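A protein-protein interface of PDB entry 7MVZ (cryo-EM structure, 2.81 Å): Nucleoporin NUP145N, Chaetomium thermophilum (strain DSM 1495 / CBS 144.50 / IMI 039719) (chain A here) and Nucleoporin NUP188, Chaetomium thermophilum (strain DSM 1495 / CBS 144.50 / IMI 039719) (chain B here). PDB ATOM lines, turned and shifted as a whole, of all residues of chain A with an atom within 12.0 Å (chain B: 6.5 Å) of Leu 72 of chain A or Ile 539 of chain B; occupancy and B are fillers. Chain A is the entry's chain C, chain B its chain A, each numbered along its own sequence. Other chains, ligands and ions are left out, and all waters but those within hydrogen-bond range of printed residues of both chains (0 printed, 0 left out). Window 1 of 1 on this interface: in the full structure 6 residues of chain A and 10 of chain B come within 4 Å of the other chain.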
ATOM      1  N   GLU A  68     -10.254  20.796  25.335  1.00  0.00           N
ATOM      2  CA  GLU A  68      -9.298  19.909  25.986  1.00  0.00           C
ATOM      3  C   GLU A  68      -9.090  18.645  25.158  1.00  0.00           C
ATOM      4  O   GLU A  68      -7.969  18.331  24.757  1.00  0.00           O
ATOM      5  CB  GLU A  68      -9.775  19.548  27.394  1.00  0.00           C
ATOM      6  CG  GLU A  68      -8.652  19.362  28.404  1.00  0.00           C
ATOM      7  CD  GLU A  68      -7.684  18.263  28.008  1.00  0.00           C
ATOM      8  OE1 GLU A  68      -6.461  18.514  28.020  1.00  0.00           O
ATOM      9  OE2 GLU A  68      -8.147  17.148  27.686  1.00  0.00           O
ATOM     10  N   ASP A  69     -10.176  17.925  24.903  1.00  0.00           N
ATOM     11  CA  ASP A  69     -10.121  16.686  24.137  1.00  0.00           C
ATOM     12  C   ASP A  69     -11.465  16.518  23.432  1.00  0.00           C
ATOM     13  O   ASP A  69     -12.208  17.488  23.250  1.00  0.00           O
ATOM     14  CB  ASP A  69      -9.766  15.506  25.060  1.00  0.00           C
ATOM     15  CG  ASP A  69      -9.130  14.349  24.313  1.00  0.00           C
ATOM     16  OD1 ASP A  69      -9.353  14.235  23.089  1.00  0.00           O
ATOM     17  OD2 ASP A  69      -8.407  13.554  24.950  1.00  0.00           O
ATOM     18  N   SER A  70     -11.781  15.287  23.033  1.00  0.00           N
ATOM     19  CA  SER A  70     -13.078  15.009  22.432  1.00  0.00           C
ATOM     20  C   SER A  70     -14.197  15.360  23.405  1.00  0.00           C
ATOM     21  O   SER A  70     -14.162  14.977  24.578  1.00  0.00           O
ATOM     22  CB  SER A  70     -13.167  13.538  22.030  1.00  0.00           C
ATOM     23  OG  SER A  70     -14.502  13.173  21.723  1.00  0.00           O
ATOM     24  N   ILE A  71     -15.195  16.093  22.911  1.00  0.00           N
ATOM     25  CA  ILE A  71     -16.278  16.555  23.768  1.00  0.00           C
ATOM     26  C   ILE A  71     -17.138  15.368  24.178  1.00  0.00           C
ATOM     27  O   ILE A  71     -17.513  14.534  23.343  1.00  0.00           O
ATOM     28  CB  ILE A  71     -17.112  17.629  23.050  1.00  0.00           C
ATOM     29  CG1 ILE A  71     -18.085  18.301  24.024  1.00  0.00           C
ATOM     30  CG2 ILE A  71     -17.876  17.021  21.881  1.00  0.00           C
ATOM     31  CD1 ILE A  71     -17.409  19.112  25.112  1.00  0.00           C
ATOM     32  N   LEU A  72     -17.456  15.290  25.468  1.00  0.00           N
ATOM     33  CA  LEU A  72     -18.368  14.280  26.002  1.00  0.00           C
ATOM     34  C   LEU A  72     -17.956  12.879  25.551  1.00  0.00           C
ATOM     35  O   LEU A  72     -18.700  12.166  24.875  1.00  0.00           O
ATOM     36  CB  LEU A  72     -19.810  14.587  25.593  1.00  0.00           C
ATOM     37  CG  LEU A  72     -20.894  13.806  26.339  1.00  0.00           C
ATOM     38  CD1 LEU A  72     -21.197  14.458  27.680  1.00  0.00           C
ATOM     39  CD2 LEU A  72     -22.153  13.698  25.494  1.00  0.00           C
ATOM     40  N   GLN A  73     -16.739  12.495  25.939  1.00  0.00           N
ATOM     41  CA  GLN A  73     -16.160  11.214  25.553  1.00  0.00           C
ATOM     42  C   GLN A  73     -17.140  10.080  25.841  1.00  0.00           C
ATOM     43  O   GLN A  73     -17.339   9.718  27.007  1.00  0.00           O
ATOM     44  CB  GLN A  73     -14.845  10.978  26.296  1.00  0.00           C
ATOM     45  CG  GLN A  73     -13.744  11.961  25.927  1.00  0.00           C
ATOM     46  CD  GLN A  73     -12.441  11.672  26.644  1.00  0.00           C
ATOM     47  OE1 GLN A  73     -12.291  10.636  27.292  1.00  0.00           O
ATOM     48  NE2 GLN A  73     -11.487  12.589  26.531  1.00  0.00           N
ATOM     49  N   PRO A  74     -17.772   9.492  24.814  1.00  0.00           N
ATOM     50  CA  PRO A  74     -18.777   8.456  25.071  1.00  0.00           C
ATOM     51  C   PRO A  74     -18.227   7.044  24.942  1.00  0.00           C
ATOM     52  O   PRO A  74     -18.920   6.072  25.260  1.00  0.00           O
ATOM     53  CB  PRO A  74     -19.832   8.746  24.001  1.00  0.00           C
ATOM     54  CG  PRO A  74     -19.020   9.269  22.826  1.00  0.00           C
ATOM     55  CD  PRO A  74     -17.699   9.805  23.376  1.00  0.00           C
ATOM     56  N   GLY A  75     -16.985   6.918  24.480  1.00  0.00           N
ATOM     57  CA  GLY A  75     -16.408   5.617  24.202  1.00  0.00           C
ATOM     58  C   GLY A  75     -15.329   5.201  25.180  1.00  0.00           C
ATOM     59  O   GLY A  75     -15.239   4.025  25.543  1.00  0.00           O
ATOM     60  N   ALA A  76     -14.499   6.153  25.606  1.00  0.00           N
ATOM     61  CA  ALA A  76     -13.427   5.852  26.546  1.00  0.00           C
ATOM     62  C   ALA A  76     -13.958   5.087  27.752  1.00  0.00           C
ATOM     63  O   ALA A  76     -15.008   5.418  28.307  1.00  0.00           O
ATOM     64  CB  ALA A  76     -12.750   7.147  27.002  1.00  0.00           C
ATOM     65  N   PHE A  77     -13.218   4.056  28.152  1.00  0.00           N
ATOM     66  CA  PHE A  77     -13.562   3.217  29.291  1.00  0.00           C
ATOM     67  C   PHE A  77     -12.519   3.398  30.384  1.00  0.00           C
ATOM     68  O   PHE A  77     -11.315   3.307  30.120  1.00  0.00           O
ATOM     69  CB  PHE A  77     -13.647   1.742  28.887  1.00  0.00           C
ATOM     70  CG  PHE A  77     -14.738   1.444  27.899  1.00  0.00           C
ATOM     71  CD1 PHE A  77     -16.040   1.245  28.327  1.00  0.00           C
ATOM     72  CD2 PHE A  77     -14.461   1.350  26.546  1.00  0.00           C
ATOM     73  CE1 PHE A  77     -17.047   0.967  27.422  1.00  0.00           C
ATOM     74  CE2 PHE A  77     -15.464   1.073  25.636  1.00  0.00           C
ATOM     75  CZ  PHE A  77     -16.759   0.880  26.076  1.00  0.00           C
ATOM     76  N   SER A  78     -12.981   3.656  31.606  1.00  0.00           N
ATOM     77  CA  SER A  78     -12.093   3.902  32.732  1.00  0.00           C
ATOM     78  C   SER A  78     -12.693   3.287  33.987  1.00  0.00           C
ATOM     79  O   SER A  78     -13.892   3.004  34.055  1.00  0.00           O
ATOM     80  CB  SER A  78     -11.851   5.404  32.942  1.00  0.00           C
ATOM     81  OG  SER A  78     -11.075   5.947  31.888  1.00  0.00           O
ATOM     82  N   ASN A  80     -13.103   4.738  36.870  1.00  0.00           N
ATOM     83  CA  ASN A  80     -14.013   5.709  37.468  1.00  0.00           C
ATOM     84  C   ASN A  80     -14.434   5.298  38.876  1.00  0.00           C
ATOM     85  O   ASN A  80     -13.656   5.406  39.824  1.00  0.00           O
ATOM     86  CB  ASN A  80     -15.250   5.886  36.587  1.00  0.00           C
ATOM     87  CG  ASN A  80     -14.931   6.543  35.260  1.00  0.00           C
ATOM     88  OD1 ASN A  80     -13.927   7.243  35.135  1.00  0.00           O
ATOM     89  ND2 ASN A  80     -15.694   6.199  34.230  1.00  0.00           N
ATOM     90  N   PHE B 406     -29.959  15.300  30.913  1.00  0.00           N
ATOM     91  CA  PHE B 406     -28.537  14.971  30.949  1.00  0.00           C
ATOM     92  C   PHE B 406     -28.223  13.962  32.053  1.00  0.00           C
ATOM     93  O   PHE B 406     -27.537  12.960  31.820  1.00  0.00           O
ATOM     94  CB  PHE B 406     -27.729  16.259  31.127  1.00  0.00           C
ATOM     95  CG  PHE B 406     -26.243  16.053  31.156  1.00  0.00           C
ATOM     96  CD1 PHE B 406     -25.519  15.983  29.977  1.00  0.00           C
ATOM     97  CD2 PHE B 406     -25.563  15.964  32.357  1.00  0.00           C
ATOM     98  CE1 PHE B 406     -24.150  15.807  29.995  1.00  0.00           C
ATOM     99  CE2 PHE B 406     -24.192  15.791  32.382  1.00  0.00           C
ATOM    100  CZ  PHE B 406     -23.486  15.711  31.199  1.00  0.00           C
ATOM    101  N   LEU B 410     -26.784  10.132  31.763  1.00  0.00           N
ATOM    102  CA  LEU B 410     -25.621   9.583  32.458  1.00  0.00           C
ATOM    103  C   LEU B 410     -25.967   8.282  33.170  1.00  0.00           C
ATOM    104  O   LEU B 410     -25.202   7.309  33.126  1.00  0.00           O
ATOM    105  CB  LEU B 410     -25.072  10.589  33.470  1.00  0.00           C
ATOM    106  CG  LEU B 410     -24.660  11.981  32.993  1.00  0.00           C
ATOM    107  CD1 LEU B 410     -24.164  12.779  34.189  1.00  0.00           C
ATOM    108  CD2 LEU B 410     -23.608  11.916  31.900  1.00  0.00           C
ATOM    109  N   GLU B 485     -27.488   9.058  24.003  1.00  0.00           N
ATOM    110  CA  GLU B 485     -26.275   9.716  23.527  1.00  0.00           C
ATOM    111  C   GLU B 485     -26.605  10.983  22.750  1.00  0.00           C
ATOM    112  O   GLU B 485     -25.951  12.016  22.929  1.00  0.00           O
ATOM    113  CB  GLU B 485     -25.461   8.752  22.663  1.00  0.00           C
ATOM    114  CG  GLU B 485     -24.837   7.601  23.438  1.00  0.00           C
ATOM    115  CD  GLU B 485     -23.759   8.058  24.402  1.00  0.00           C
ATOM    116  OE1 GLU B 485     -23.386   9.250  24.359  1.00  0.00           O
ATOM    117  OE2 GLU B 485     -23.285   7.226  25.203  1.00  0.00           O
ATOM    118  N   ALA B 488     -27.659  13.664  25.248  1.00  0.00           N
ATOM    119  CA  ALA B 488     -26.514  14.261  25.927  1.00  0.00           C
ATOM    120  C   ALA B 488     -25.733  15.175  24.991  1.00  0.00           C
ATOM    121  O   ALA B 488     -25.266  16.244  25.403  1.00  0.00           O
ATOM    122  CB  ALA B 488     -25.608  13.166  26.488  1.00  0.00           C
ATOM    123  N   MET B 489     -25.574  14.767  23.730  1.00  0.00           N
ATOM    124  CA  MET B 489     -24.906  15.618  22.751  1.00  0.00           C
ATOM    125  C   MET B 489     -25.634  16.948  22.598  1.00  0.00           C
ATOM    126  O   MET B 489     -25.013  18.017  22.627  1.00  0.00           O
ATOM    127  CB  MET B 489     -24.818  14.895  21.407  1.00  0.00           C
ATOM    128  CG  MET B 489     -24.102  15.685  20.322  1.00  0.00           C
ATOM    129  SD  MET B 489     -23.795  14.710  18.838  1.00  0.00           S
ATOM    130  CE  MET B 489     -23.124  15.961  17.745  1.00  0.00           C
ATOM    131  N   THR B 492     -25.120  19.129  25.711  1.00  0.00           N
ATOM    132  CA  THR B 492     -23.791  19.708  25.872  1.00  0.00           C
ATOM    133  C   THR B 492     -23.418  20.651  24.734  1.00  0.00           C
ATOM    134  O   THR B 492     -22.475  21.434  24.884  1.00  0.00           O
ATOM    135  CB  THR B 492     -22.739  18.598  25.986  1.00  0.00           C
ATOM    136  OG1 THR B 492     -21.475  19.166  26.353  1.00  0.00           O
ATOM    137  CG2 THR B 492     -22.588  17.843  24.668  1.00  0.00           C
ATOM    138  N   TYR B 498     -24.965  23.770  30.738  1.00  0.00           N
ATOM    139  CA  TYR B 498     -24.183  24.512  31.721  1.00  0.00           C
ATOM    140  C   TYR B 498     -24.754  25.907  31.942  1.00  0.00           C
ATOM    141  O   TYR B 498     -24.816  26.385  33.081  1.00  0.00           O
ATOM    142  CB  TYR B 498     -22.724  24.589  31.272  1.00  0.00           C
ATOM    143  CG  TYR B 498     -22.066  23.234  31.106  1.00  0.00           C
ATOM    144  CD1 TYR B 498     -22.379  22.179  31.953  1.00  0.00           C
ATOM    145  CD2 TYR B 498     -21.148  23.007  30.092  1.00  0.00           C
ATOM    146  CE1 TYR B 498     -21.785  20.942  31.803  1.00  0.00           C
ATOM    147  CE2 TYR B 498     -20.548  21.772  29.932  1.00  0.00           C
ATOM    148  CZ  TYR B 498     -20.871  20.743  30.791  1.00  0.00           C
ATOM    149  OH  TYR B 498     -20.279  19.512  30.638  1.00  0.00           O
ATOM    150  N   SER B 535     -20.487  14.091  36.825  1.00  0.00           N
ATOM    151  CA  SER B 535     -20.267  14.367  35.380  1.00  0.00           C
ATOM    152  C   SER B 535     -18.855  14.905  35.133  1.00  0.00           C
ATOM    153  O   SER B 535     -18.526  15.125  33.953  1.00  0.00           O
ATOM    154  CB  SER B 535     -21.299  15.310  34.824  1.00  0.00           C
ATOM    155  OG  SER B 535     -21.344  16.502  35.593  1.00  0.00           O
ATOM    156  N   ALA B 536     -18.036  15.092  36.173  1.00  0.00           N
ATOM    157  CA  ALA B 536     -16.657  15.606  36.006  1.00  0.00           C
ATOM    158  C   ALA B 536     -15.823  14.521  35.350  1.00  0.00           C
ATOM    159  O   ALA B 536     -15.271  14.772  34.263  1.00  0.00           O
ATOM    160  CB  ALA B 536     -16.004  16.014  37.305  1.00  0.00           C
ATOM    161  N   TYR B 537     -15.781  13.339  35.964  1.00  0.00           N
ATOM    162  CA  TYR B 537     -14.892  12.296  35.466  1.00  0.00           C
ATOM    163  C   TYR B 537     -15.356  11.701  34.142  1.00  0.00           C
ATOM    164  O   TYR B 537     -14.584  10.975  33.509  1.00  0.00           O
ATOM    165  CB  TYR B 537     -14.732  11.179  36.502  1.00  0.00           C
ATOM    166  CG  TYR B 537     -16.000  10.429  36.842  1.00  0.00           C
ATOM    167  CD1 TYR B 537     -16.401   9.330  36.094  1.00  0.00           C
ATOM    168  CD2 TYR B 537     -16.761  10.777  37.950  1.00  0.00           C
ATOM    169  CE1 TYR B 537     -17.546   8.625  36.414  1.00  0.00           C
ATOM    170  CE2 TYR B 537     -17.907  10.076  38.279  1.00  0.00           C
ATOM    171  CZ  TYR B 537     -18.295   9.003  37.506  1.00  0.00           C
ATOM    172  OH  TYR B 537     -19.435   8.305  37.830  1.00  0.00           O
ATOM    173  N   LEU B 538     -16.585  11.984  33.710  1.00  0.00           N
ATOM    174  CA  LEU B 538     -17.088  11.468  32.430  1.00  0.00           C
ATOM    175  C   LEU B 538     -16.667  12.371  31.274  1.00  0.00           C
ATOM    176  O   LEU B 538     -15.891  11.962  30.406  1.00  0.00           O
ATOM    177  CB  LEU B 538     -18.608  11.316  32.495  1.00  0.00           C
ATOM    178  CG  LEU B 538     -19.089  10.025  33.159  1.00  0.00           C
ATOM    179  CD1 LEU B 538     -20.514  10.182  33.653  1.00  0.00           C
ATOM    180  CD2 LEU B 538     -18.978   8.856  32.196  1.00  0.00           C
ATOM    181  N   ILE B 539     -17.174  13.600  31.254  1.00  0.00           N
ATOM    182  CA  ILE B 539     -16.768  14.587  30.255  1.00  0.00           C
ATOM    183  C   ILE B 539     -15.454  15.184  30.750  1.00  0.00           C
ATOM    184  O   ILE B 539     -15.306  15.400  31.961  1.00  0.00           O
ATOM    185  CB  ILE B 539     -17.873  15.645  30.064  1.00  0.00           C
ATOM    186  CG1 ILE B 539     -17.550  16.600  28.915  1.00  0.00           C
ATOM    187  CG2 ILE B 539     -18.087  16.442  31.350  1.00  0.00           C
ATOM    188  CD1 ILE B 539     -18.720  17.459  28.475  1.00  0.00           C
ATOM    189  N   PRO B 540     -14.479  15.472  29.886  1.00  0.00           N
ATOM    190  CA  PRO B 540     -13.172  15.910  30.387  1.00  0.00           C
ATOM    191  C   PRO B 540     -13.226  17.320  30.954  1.00  0.00           C
ATOM    192  O   PRO B 540     -14.215  18.046  30.831  1.00  0.00           O
ATOM    193  CB  PRO B 540     -12.276  15.808  29.153  1.00  0.00           C
ATOM    194  CG  PRO B 540     -13.172  16.126  28.034  1.00  0.00           C
ATOM    195  CD  PRO B 540     -14.543  15.593  28.416  1.00  0.00           C
ATOM    196  N   TYR B 541     -12.121  17.704  31.589  1.00  0.00           N
ATOM    197  CA  TYR B 541     -11.982  19.057  32.109  1.00  0.00           C
ATOM    198  C   TYR B 541     -12.030  20.066  30.971  1.00  0.00           C
ATOM    199  O   TYR B 541     -11.349  19.907  29.953  1.00  0.00           O
ATOM    200  CB  TYR B 541     -10.667  19.180  32.881  1.00  0.00           C
ATOM    201  CG  TYR B 541     -10.500  20.480  33.636  1.00  0.00           C
ATOM    202  CD1 TYR B 541     -10.008  21.616  33.005  1.00  0.00           C
ATOM    203  CD2 TYR B 541     -10.816  20.566  34.985  1.00  0.00           C
ATOM    204  CE1 TYR B 541      -9.846  22.802  33.695  1.00  0.00           C
ATOM    205  CE2 TYR B 541     -10.658  21.747  35.682  1.00  0.00           C
ATOM    206  CZ  TYR B 541     -10.172  22.862  35.033  1.00  0.00           C
ATOM    207  OH  TYR B 541     -10.014  24.040  35.725  1.00  0.00           O
ATOM    208  N   GLN B 542     -12.839  21.108  31.146  1.00  0.00           N
ATOM    209  CA  GLN B 542     -13.033  22.107  30.104  1.00  0.00           C
ATOM    210  C   GLN B 542     -13.539  23.389  30.749  1.00  0.00           C
ATOM    211  O   GLN B 542     -14.047  23.380  31.873  1.00  0.00           O
ATOM    212  CB  GLN B 542     -14.008  21.606  29.031  1.00  0.00           C
ATOM    213  CG  GLN B 542     -14.145  22.519  27.825  1.00  0.00           C
ATOM    214  CD  GLN B 542     -14.985  21.904  26.724  1.00  0.00           C
ATOM    215  OE1 GLN B 542     -15.399  20.748  26.815  1.00  0.00           O
ATOM    216  NE2 GLN B 542     -15.245  22.677  25.676  1.00  0.00           N
ATOM    217  N   PRO B 545     -17.639  23.669  31.961  1.00  0.00           N
ATOM    218  CA  PRO B 545     -17.995  23.146  33.292  1.00  0.00           C
ATOM    219  C   PRO B 545     -17.373  23.936  34.427  1.00  0.00           C
ATOM    220  O   PRO B 545     -17.981  24.054  35.499  1.00  0.00           O
ATOM    221  CB  PRO B 545     -17.480  21.698  33.262  1.00  0.00           C
ATOM    222  CG  PRO B 545     -16.653  21.568  32.023  1.00  0.00           C
ATOM    223  CD  PRO B 545     -17.097  22.626  31.076  1.00  0.00           C
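Printed residues of chain A that touch a printed residue of chain B: Glu 68, Ser 70, Ile 71, Leu 72, Pro 74 and Asn 80. Along chain A the printed residues that touch a printed residue of chain B span positions 68 to 80. Among the printed residues, 10 pairs touch across the chains. Among the printed residues, no Asp or Glu carboxylate lies within 4 Å of a Lys or Arg side-chain nitrogen of the other chain.
Of the printed residues of chain B, Glu 68 of chain A touches Tyr 541 (3.0 Å). Asp 69 of chain A touches none of the printed residues of chain B. Of the printed residues of chain B, Ser 70 of chain A touches Pro 540. Of the printed residues of chain B, Ile 71 of chain A touches Ile 539 (3.97 Å) and Gln 542 (3.1 Å). Of the printed residues of chain B, Leu 72 of chain A touches Phe 406, Ala 488, Met 489 and Ile 539. Glu 485 of chain B touches just one residue of chain A: Pro 74. Of chain A, only Leu 72 comes within 4 Å of Ala 488 of chain B. Tyr 498 of chain B touches none of the printed residues of chain A. No residue of chain A comes within 4 Å of Ala 536 of chain B. No residue of chain A comes within 4 Å of Leu 538 of chain B. Printed residues of chain A within 4 Å of Ile 539 of chain B: Ile 71 and Leu 72. Pro 540 of chain B touches just one residue of chain A: Ser 70 (3.8 Å). Of the printed residues of chain A, Tyr 541 of chain B touches Glu 68. Printed residues of chain A within 4 Å of Gln 542 of chain B: Ile 71 (3.1 Å). The nearest residue of chain A that does not touch Ile 539 of chain B is Gln 73 of chain A (4.8 Å). The nearest printed residue of chain A that does not touch Gln 542 of chain B is Glu 68 of chain A (4.9 Å).
Among the printed residues, merely in contact across the chains: Glu 68 of chain A with Tyr 541 of chain B, Ser 70 of chain A with Pro 540 of chain B, Ile 71 of chain A with Ile 539 of chain B, Ile 71 of chain A with Gln 542 of chain B, Leu 72 of chain A with Phe 406 of chain B, Leu 72 of chain A with Ala 488 of chain B, Leu 72 of chain A with Met 489 of chain B, Leu 72 of chain A with Ile 539 of chain B, Pro 74 of chain A with Glu 485 of chain B and Asn 80 of chain A with Tyr 537 of chain B.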
